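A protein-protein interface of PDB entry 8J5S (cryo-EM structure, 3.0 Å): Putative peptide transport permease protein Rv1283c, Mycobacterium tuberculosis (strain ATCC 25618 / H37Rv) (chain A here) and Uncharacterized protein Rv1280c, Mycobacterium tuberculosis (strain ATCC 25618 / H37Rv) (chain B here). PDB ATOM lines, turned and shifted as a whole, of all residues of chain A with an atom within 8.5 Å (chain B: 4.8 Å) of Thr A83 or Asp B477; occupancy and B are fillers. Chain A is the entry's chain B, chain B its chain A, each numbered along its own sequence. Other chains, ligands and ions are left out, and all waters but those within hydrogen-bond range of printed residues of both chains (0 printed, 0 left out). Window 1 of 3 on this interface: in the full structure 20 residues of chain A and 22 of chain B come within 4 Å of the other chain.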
ATOM      1  N   PRO A  33     -22.526  -1.151  32.650  1.00  0.00           N
ATOM      2  CA  PRO A  33     -23.330  -0.118  31.997  1.00  0.00           C
ATOM      3  C   PRO A  33     -23.091   1.280  32.527  1.00  0.00           C
ATOM      4  O   PRO A  33     -23.454   2.247  31.851  1.00  0.00           O
ATOM      5  CB  PRO A  33     -24.760  -0.578  32.272  1.00  0.00           C
ATOM      6  CG  PRO A  33     -24.668  -1.331  33.515  1.00  0.00           C
ATOM      7  CD  PRO A  33     -23.338  -1.999  33.532  1.00  0.00           C
ATOM      8  N   SER A  36     -19.379   4.429  31.138  1.00  0.00           N
ATOM      9  CA  SER A  36     -19.367   5.652  30.352  1.00  0.00           C
ATOM     10  C   SER A  36     -19.992   6.817  31.087  1.00  0.00           C
ATOM     11  O   SER A  36     -19.826   7.959  30.656  1.00  0.00           O
ATOM     12  CB  SER A  36     -20.097   5.441  29.030  1.00  0.00           C
ATOM     13  OG  SER A  36     -20.372   6.681  28.410  1.00  0.00           O
ATOM     14  N   LEU A  37     -20.771   6.517  32.122  1.00  0.00           N
ATOM     15  CA  LEU A  37     -21.448   7.535  32.917  1.00  0.00           C
ATOM     16  C   LEU A  37     -20.527   7.965  34.042  1.00  0.00           C
ATOM     17  O   LEU A  37     -20.382   9.153  34.327  1.00  0.00           O
ATOM     18  CB  LEU A  37     -22.759   6.987  33.485  1.00  0.00           C
ATOM     19  CG  LEU A  37     -23.620   7.942  34.315  1.00  0.00           C
ATOM     20  CD1 LEU A  37     -24.961   7.305  34.648  1.00  0.00           C
ATOM     21  CD2 LEU A  37     -22.897   8.372  35.582  1.00  0.00           C
ATOM     22  N   ARG A  40     -17.016  10.501  33.296  1.00  0.00           N
ATOM     23  CA  ARG A  40     -17.346  11.772  32.628  1.00  0.00           C
ATOM     24  C   ARG A  40     -16.348  12.714  33.265  1.00  0.00           C
ATOM     25  O   ARG A  40     -15.969  12.446  34.394  1.00  0.00           O
ATOM     26  CB  ARG A  40     -18.780  12.180  32.933  1.00  0.00           C
ATOM     27  CG  ARG A  40     -19.672  12.247  31.710  1.00  0.00           C
ATOM     28  CD  ARG A  40     -20.685  11.130  31.707  1.00  0.00           C
ATOM     29  NE  ARG A  40     -21.911  11.592  32.325  1.00  0.00           N
ATOM     30  CZ  ARG A  40     -23.101  11.514  31.757  1.00  0.00           C
ATOM     31  NH1 ARG A  40     -23.296  10.683  30.752  1.00  0.00           N
ATOM     32  NH2 ARG A  40     -24.090  12.267  32.197  1.00  0.00           N
ATOM     33  N   LYS A  52     -29.363   6.384  38.555  1.00  0.00           N
ATOM     34  CA  LYS A  52     -29.223   5.541  37.379  1.00  0.00           C
ATOM     35  C   LYS A  52     -28.959   4.093  37.753  1.00  0.00           C
ATOM     36  O   LYS A  52     -29.337   3.190  37.005  1.00  0.00           O
ATOM     37  CB  LYS A  52     -28.108   6.066  36.486  1.00  0.00           C
ATOM     38  CG  LYS A  52     -28.248   5.662  35.037  1.00  0.00           C
ATOM     39  CD  LYS A  52     -29.202   6.585  34.310  1.00  0.00           C
ATOM     40  CE  LYS A  52     -29.745   5.932  33.062  1.00  0.00           C
ATOM     41  NZ  LYS A  52     -31.032   5.232  33.305  1.00  0.00           N
ATOM     42  N   ASP A  55     -32.544   2.909  38.586  1.00  0.00           N
ATOM     43  CA  ASP A  55     -33.425   2.755  37.439  1.00  0.00           C
ATOM     44  C   ASP A  55     -33.097   1.527  36.613  1.00  0.00           C
ATOM     45  O   ASP A  55     -33.885   1.164  35.736  1.00  0.00           O
ATOM     46  CB  ASP A  55     -33.362   3.996  36.554  1.00  0.00           C
ATOM     47  CG  ASP A  55     -33.944   5.215  37.226  1.00  0.00           C
ATOM     48  OD1 ASP A  55     -34.886   5.059  38.027  1.00  0.00           O
ATOM     49  OD2 ASP A  55     -33.458   6.332  36.954  1.00  0.00           O
ATOM     50  N   LEU A  56     -31.961   0.887  36.858  1.00  0.00           N
ATOM     51  CA  LEU A  56     -31.591  -0.336  36.170  1.00  0.00           C
ATOM     52  C   LEU A  56     -31.567  -1.545  37.092  1.00  0.00           C
ATOM     53  O   LEU A  56     -31.290  -2.655  36.630  1.00  0.00           O
ATOM     54  CB  LEU A  56     -30.228  -0.159  35.501  1.00  0.00           C
ATOM     55  CG  LEU A  56     -30.144   0.976  34.490  1.00  0.00           C
ATOM     56  CD1 LEU A  56     -28.716   1.166  34.018  1.00  0.00           C
ATOM     57  CD2 LEU A  56     -31.062   0.689  33.325  1.00  0.00           C
ATOM     58  N   THR A  80     -36.072  -0.092  30.755  1.00  0.00           N
ATOM     59  CA  THR A  80     -35.485   0.970  29.966  1.00  0.00           C
ATOM     60  C   THR A  80     -34.247   0.469  29.234  1.00  0.00           C
ATOM     61  O   THR A  80     -33.793  -0.659  29.419  1.00  0.00           O
ATOM     62  CB  THR A  80     -35.108   2.148  30.856  1.00  0.00           C
ATOM     63  OG1 THR A  80     -33.848   1.885  31.482  1.00  0.00           O
ATOM     64  CG2 THR A  80     -36.155   2.364  31.928  1.00  0.00           C
ATOM     65  N   THR A  81     -33.713   1.318  28.368  1.00  0.00           N
ATOM     66  CA  THR A  81     -32.363   1.136  27.868  1.00  0.00           C
ATOM     67  C   THR A  81     -31.423   1.965  28.739  1.00  0.00           C
ATOM     68  O   THR A  81     -31.822   2.510  29.771  1.00  0.00           O
ATOM     69  CB  THR A  81     -32.257   1.520  26.396  1.00  0.00           C
ATOM     70  OG1 THR A  81     -32.126   2.937  26.279  1.00  0.00           O
ATOM     71  CG2 THR A  81     -33.466   1.061  25.630  1.00  0.00           C
ATOM     72  N   ILE A  82     -30.156   2.069  28.333  1.00  0.00           N
ATOM     73  CA  ILE A  82     -29.194   2.847  29.103  1.00  0.00           C
ATOM     74  C   ILE A  82     -29.635   4.296  29.195  1.00  0.00           C
ATOM     75  O   ILE A  82     -29.364   4.975  30.190  1.00  0.00           O
ATOM     76  CB  ILE A  82     -27.793   2.714  28.483  1.00  0.00           C
ATOM     77  CG1 ILE A  82     -27.239   1.324  28.750  1.00  0.00           C
ATOM     78  CG2 ILE A  82     -26.844   3.746  29.049  1.00  0.00           C
ATOM     79  CD1 ILE A  82     -26.773   1.155  30.147  1.00  0.00           C
ATOM     80  N   THR A  83     -30.331   4.789  28.178  1.00  0.00           N
ATOM     81  CA  THR A  83     -30.805   6.163  28.153  1.00  0.00           C
ATOM     82  C   THR A  83     -32.162   6.350  28.815  1.00  0.00           C
ATOM     83  O   THR A  83     -32.563   7.493  29.050  1.00  0.00           O
ATOM     84  CB  THR A  83     -30.892   6.653  26.713  1.00  0.00           C
ATOM     85  OG1 THR A  83     -32.117   6.187  26.136  1.00  0.00           O
ATOM     86  CG2 THR A  83     -29.733   6.114  25.908  1.00  0.00           C
ATOM     87  N   GLY A  84     -32.875   5.275  29.127  1.00  0.00           N
ATOM     88  CA  GLY A  84     -34.198   5.374  29.700  1.00  0.00           C
ATOM     89  C   GLY A  84     -35.334   5.065  28.749  1.00  0.00           C
ATOM     90  O   GLY A  84     -36.480   4.961  29.195  1.00  0.00           O
ATOM     91  N   GLN A  85     -35.054   4.924  27.459  1.00  0.00           N
ATOM     92  CA  GLN A  85     -36.089   4.565  26.506  1.00  0.00           C
ATOM     93  C   GLN A  85     -36.577   3.143  26.766  1.00  0.00           C
ATOM     94  O   GLN A  85     -35.799   2.280  27.168  1.00  0.00           O
ATOM     95  CB  GLN A  85     -35.554   4.673  25.084  1.00  0.00           C
ATOM     96  CG  GLN A  85     -35.236   6.088  24.661  1.00  0.00           C
ATOM     97  CD  GLN A  85     -36.476   6.945  24.570  1.00  0.00           C
ATOM     98  OE1 GLN A  85     -36.605   7.952  25.263  1.00  0.00           O
ATOM     99  NE2 GLN A  85     -37.408   6.541  23.717  1.00  0.00           N
ATOM    100  N   PRO A  86     -37.861   2.871  26.552  1.00  0.00           N
ATOM    101  CA  PRO A  86     -38.370   1.514  26.769  1.00  0.00           C
ATOM    102  C   PRO A  86     -37.854   0.547  25.718  1.00  0.00           C
ATOM    103  O   PRO A  86     -37.455   0.931  24.618  1.00  0.00           O
ATOM    104  CB  PRO A  86     -39.889   1.679  26.671  1.00  0.00           C
ATOM    105  CG  PRO A  86     -40.136   3.134  26.783  1.00  0.00           C
ATOM    106  CD  PRO A  86     -38.938   3.806  26.210  1.00  0.00           C
ATOM    107  N   ARG A 283     -25.902  -3.015  18.480  1.00  0.00           N
ATOM    108  CA  ARG A 283     -26.043  -1.758  19.201  1.00  0.00           C
ATOM    109  C   ARG A 283     -25.984  -1.968  20.709  1.00  0.00           C
ATOM    110  O   ARG A 283     -25.256  -1.268  21.419  1.00  0.00           O
ATOM    111  CB  ARG A 283     -27.355  -1.097  18.789  1.00  0.00           C
ATOM    112  CG  ARG A 283     -27.612   0.262  19.375  1.00  0.00           C
ATOM    113  CD  ARG A 283     -26.549   1.277  18.975  1.00  0.00           C
ATOM    114  NE  ARG A 283     -26.983   2.667  19.131  1.00  0.00           N
ATOM    115  CZ  ARG A 283     -27.530   3.195  20.227  1.00  0.00           C
ATOM    116  NH1 ARG A 283     -27.879   4.470  20.230  1.00  0.00           N
ATOM    117  NH2 ARG A 283     -27.722   2.475  21.322  1.00  0.00           N
ATOM    118  N   THR A 287     -23.039  -0.536  23.235  1.00  0.00           N
ATOM    119  CA  THR A 287     -23.339   0.384  24.324  1.00  0.00           C
ATOM    120  C   THR A 287     -23.423  -0.300  25.678  1.00  0.00           C
ATOM    121  O   THR A 287     -23.676   0.376  26.677  1.00  0.00           O
ATOM    122  CB  THR A 287     -24.641   1.137  24.058  1.00  0.00           C
ATOM    123  OG1 THR A 287     -25.754   0.320  24.419  1.00  0.00           O
ATOM    124  CG2 THR A 287     -24.746   1.524  22.607  1.00  0.00           C
ATOM    125  N   ASP A 289     -25.583  -2.644  27.125  1.00  0.00           N
ATOM    126  CA  ASP A 289     -26.912  -2.581  27.708  1.00  0.00           C
ATOM    127  C   ASP A 289     -27.384  -3.986  28.043  1.00  0.00           C
ATOM    128  O   ASP A 289     -27.395  -4.863  27.178  1.00  0.00           O
ATOM    129  CB  ASP A 289     -27.899  -1.913  26.758  1.00  0.00           C
ATOM    130  CG  ASP A 289     -29.191  -1.552  27.438  1.00  0.00           C
ATOM    131  OD1 ASP A 289     -29.342  -1.856  28.638  1.00  0.00           O
ATOM    132  OD2 ASP A 289     -30.063  -0.954  26.784  1.00  0.00           O
ATOM    133  N   ILE A 292     -31.392  -4.839  26.570  1.00  0.00           N
ATOM    134  CA  ILE A 292     -31.508  -5.140  25.147  1.00  0.00           C
ATOM    135  C   ILE A 292     -30.965  -6.528  24.855  1.00  0.00           C
ATOM    136  O   ILE A 292     -31.601  -7.338  24.172  1.00  0.00           O
ATOM    137  CB  ILE A 292     -30.781  -4.073  24.316  1.00  0.00           C
ATOM    138  CG1 ILE A 292     -31.555  -2.763  24.332  1.00  0.00           C
ATOM    139  CG2 ILE A 292     -30.569  -4.564  22.912  1.00  0.00           C
ATOM    140  CD1 ILE A 292     -30.742  -1.597  23.871  1.00  0.00           C
ATOM    141  N   GLY B 473     -27.660  10.299  19.515  1.00  0.00           N
ATOM    142  CA  GLY B 473     -27.155  10.739  20.792  1.00  0.00           C
ATOM    143  C   GLY B 473     -25.648  10.652  20.830  1.00  0.00           C
ATOM    144  O   GLY B 473     -25.078  10.030  21.723  1.00  0.00           O
ATOM    145  N   PHE B 474     -24.992  11.194  19.811  1.00  0.00           N
ATOM    146  CA  PHE B 474     -23.549  11.343  19.860  1.00  0.00           C
ATOM    147  C   PHE B 474     -23.208  12.575  20.676  1.00  0.00           C
ATOM    148  O   PHE B 474     -22.464  12.500  21.659  1.00  0.00           O
ATOM    149  CB  PHE B 474     -22.990  11.417  18.434  1.00  0.00           C
ATOM    150  CG  PHE B 474     -21.528  11.722  18.356  1.00  0.00           C
ATOM    151  CD1 PHE B 474     -21.085  12.995  18.080  1.00  0.00           C
ATOM    152  CD2 PHE B 474     -20.596  10.739  18.571  1.00  0.00           C
ATOM    153  CE1 PHE B 474     -19.743  13.274  18.009  1.00  0.00           C
ATOM    154  CE2 PHE B 474     -19.255  11.017  18.507  1.00  0.00           C
ATOM    155  CZ  PHE B 474     -18.830  12.286  18.226  1.00  0.00           C
ATOM    156  N   PHE B 475     -23.844  13.687  20.340  1.00  0.00           N
ATOM    157  CA  PHE B 475     -23.680  14.895  21.123  1.00  0.00           C
ATOM    158  C   PHE B 475     -24.398  14.779  22.457  1.00  0.00           C
ATOM    159  O   PHE B 475     -23.751  14.757  23.503  1.00  0.00           O
ATOM    160  CB  PHE B 475     -24.173  16.094  20.319  1.00  0.00           C
ATOM    161  CG  PHE B 475     -23.212  16.516  19.261  1.00  0.00           C
ATOM    162  CD1 PHE B 475     -23.151  15.847  18.054  1.00  0.00           C
ATOM    163  CD2 PHE B 475     -22.335  17.547  19.485  1.00  0.00           C
ATOM    164  CE1 PHE B 475     -22.253  16.215  17.097  1.00  0.00           C
ATOM    165  CE2 PHE B 475     -21.439  17.912  18.528  1.00  0.00           C
ATOM    166  CZ  PHE B 475     -21.401  17.248  17.333  1.00  0.00           C
ATOM    167  N   SER B 476     -25.725  14.642  22.432  1.00  0.00           N
ATOM    168  CA  SER B 476     -26.517  14.726  23.655  1.00  0.00           C
ATOM    169  C   SER B 476     -26.080  13.710  24.695  1.00  0.00           C
ATOM    170  O   SER B 476     -26.270  13.932  25.894  1.00  0.00           O
ATOM    171  CB  SER B 476     -27.993  14.530  23.329  1.00  0.00           C
ATOM    172  OG  SER B 476     -28.198  13.309  22.651  1.00  0.00           O
ATOM    173  N   ASP B 477     -25.494  12.600  24.264  1.00  0.00           N
ATOM    174  CA  ASP B 477     -25.071  11.565  25.190  1.00  0.00           C
ATOM    175  C   ASP B 477     -23.586  11.590  25.504  1.00  0.00           C
ATOM    176  O   ASP B 477     -23.198  11.070  26.551  1.00  0.00           O
ATOM    177  CB  ASP B 477     -25.425  10.181  24.644  1.00  0.00           C
ATOM    178  CG  ASP B 477     -26.715   9.642  25.207  1.00  0.00           C
ATOM    179  OD1 ASP B 477     -27.421  10.392  25.907  1.00  0.00           O
ATOM    180  OD2 ASP B 477     -27.027   8.463  24.943  1.00  0.00           O
ATOM    181  N   TYR B 478     -22.735  12.162  24.652  1.00  0.00           N
ATOM    182  CA  TYR B 478     -21.323  12.065  24.984  1.00  0.00           C
ATOM    183  C   TYR B 478     -20.606  13.405  25.010  1.00  0.00           C
ATOM    184  O   TYR B 478     -19.707  13.602  25.826  1.00  0.00           O
ATOM    185  CB  TYR B 478     -20.638  11.112  24.018  1.00  0.00           C
ATOM    186  CG  TYR B 478     -21.270   9.747  23.999  1.00  0.00           C
ATOM    187  CD1 TYR B 478     -22.292   9.453  23.122  1.00  0.00           C
ATOM    188  CD2 TYR B 478     -20.860   8.757  24.870  1.00  0.00           C
ATOM    189  CE1 TYR B 478     -22.878   8.215  23.104  1.00  0.00           C
ATOM    190  CE2 TYR B 478     -21.442   7.514  24.859  1.00  0.00           C
ATOM    191  CZ  TYR B 478     -22.451   7.250  23.975  1.00  0.00           C
ATOM    192  OH  TYR B 478     -23.039   6.011  23.954  1.00  0.00           O
ATOM    193  N   VAL B 479     -20.987  14.336  24.148  1.00  0.00           N
ATOM    194  CA  VAL B 479     -20.237  15.576  24.016  1.00  0.00           C
ATOM    195  C   VAL B 479     -20.774  16.653  24.943  1.00  0.00           C
ATOM    196  O   VAL B 479     -20.009  17.322  25.637  1.00  0.00           O
ATOM    197  CB  VAL B 479     -20.234  16.038  22.545  1.00  0.00           C
ATOM    198  CG1 VAL B 479     -19.368  17.244  22.376  1.00  0.00           C
ATOM    199  CG2 VAL B 479     -19.743  14.931  21.651  1.00  0.00           C
ATOM    200  N   VAL B 481     -22.160  16.266  27.662  1.00  0.00           N
ATOM    201  CA  VAL B 481     -22.092  15.819  29.047  1.00  0.00           C
ATOM    202  C   VAL B 481     -20.665  15.681  29.563  1.00  0.00           C
ATOM    203  O   VAL B 481     -20.466  15.659  30.785  1.00  0.00           O
ATOM    204  CB  VAL B 481     -22.844  14.489  29.213  1.00  0.00           C
ATOM    205  CG1 VAL B 481     -24.262  14.629  28.719  1.00  0.00           C
ATOM    206  CG2 VAL B 481     -22.142  13.411  28.453  1.00  0.00           C
ATOM    207  N   ALA B 483     -18.299  13.175  28.357  1.00  0.00           N
ATOM    208  CA  ALA B 483     -17.859  11.784  28.396  1.00  0.00           C
ATOM    209  C   ALA B 483     -16.820  11.507  27.312  1.00  0.00           C
ATOM    210  O   ALA B 483     -16.991  10.651  26.451  1.00  0.00           O
ATOM    211  CB  ALA B 483     -19.056  10.852  28.263  1.00  0.00           C
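CE2 of Tyr B478 touches OG of Ser A36 (3.8 Å). Ser A36 touches Ala B483 (O to CB, 3.8 Å). Val B481 touches Arg A40 (O to CG, 3.6 Å). CG of Arg A40 touches N of Ala B483, 3.7 Å away. Asp B477 touches Thr A83.
The backbone NH (N) of Ala B483 lies within hydrogen-bond range of the backbone carbonyl oxygen (O) of Tyr B478, at 2.9 Å. The side-chain hydroxyl of Thr A81 sits close to the backbone NH of Thr A83 (3.2 Å). N of Gln A85 sits close to OG1 of Thr A83, at 3.5 Å.
Of chain B, only Asp B477 (3.7 Å) comes within 4 Å of Thr A83. Of chain A, only Thr A83 comes within 4 Å of Asp B477. No residue of chain A comes within 4 Å of Ser B476. Of the printed residues of chain A, Tyr B478 touches Ser A36. Of the printed residues of chain B, Arg A40 touches Val B481 (3.6 Å) and Ala B483 (3.7 Å). Printed residues of chain A within 4 Å of Ala B483: Ser A36 and Arg A40. Of the printed residues of chain A, Val B481 touches Arg A40. Of the printed residues of chain B, Ser A36 touches Tyr B478 and Ala B483. Phe B474 touches none of the printed residues of chain A. The nearest printed residue of chain A that does not touch Ala B483 is Leu A37 (6.1 Å).
Printed residues of chain A that touch a printed residue of chain B: Ser A36, Arg A40 and Thr A83. Printed residues of chain B that touch a printed residue of chain A: Asp B477, Tyr B478, Val B481 and Ala B483. Hydrophobic or aromatic side chains of chain B within 4 Å of the printed part of chain A: Tyr B478, Val B481 and Ala B483. Among the printed residues, no Asp or Glu carboxylate lies within 4 Å of a Lys or Arg side-chain nitrogen of the other chain.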
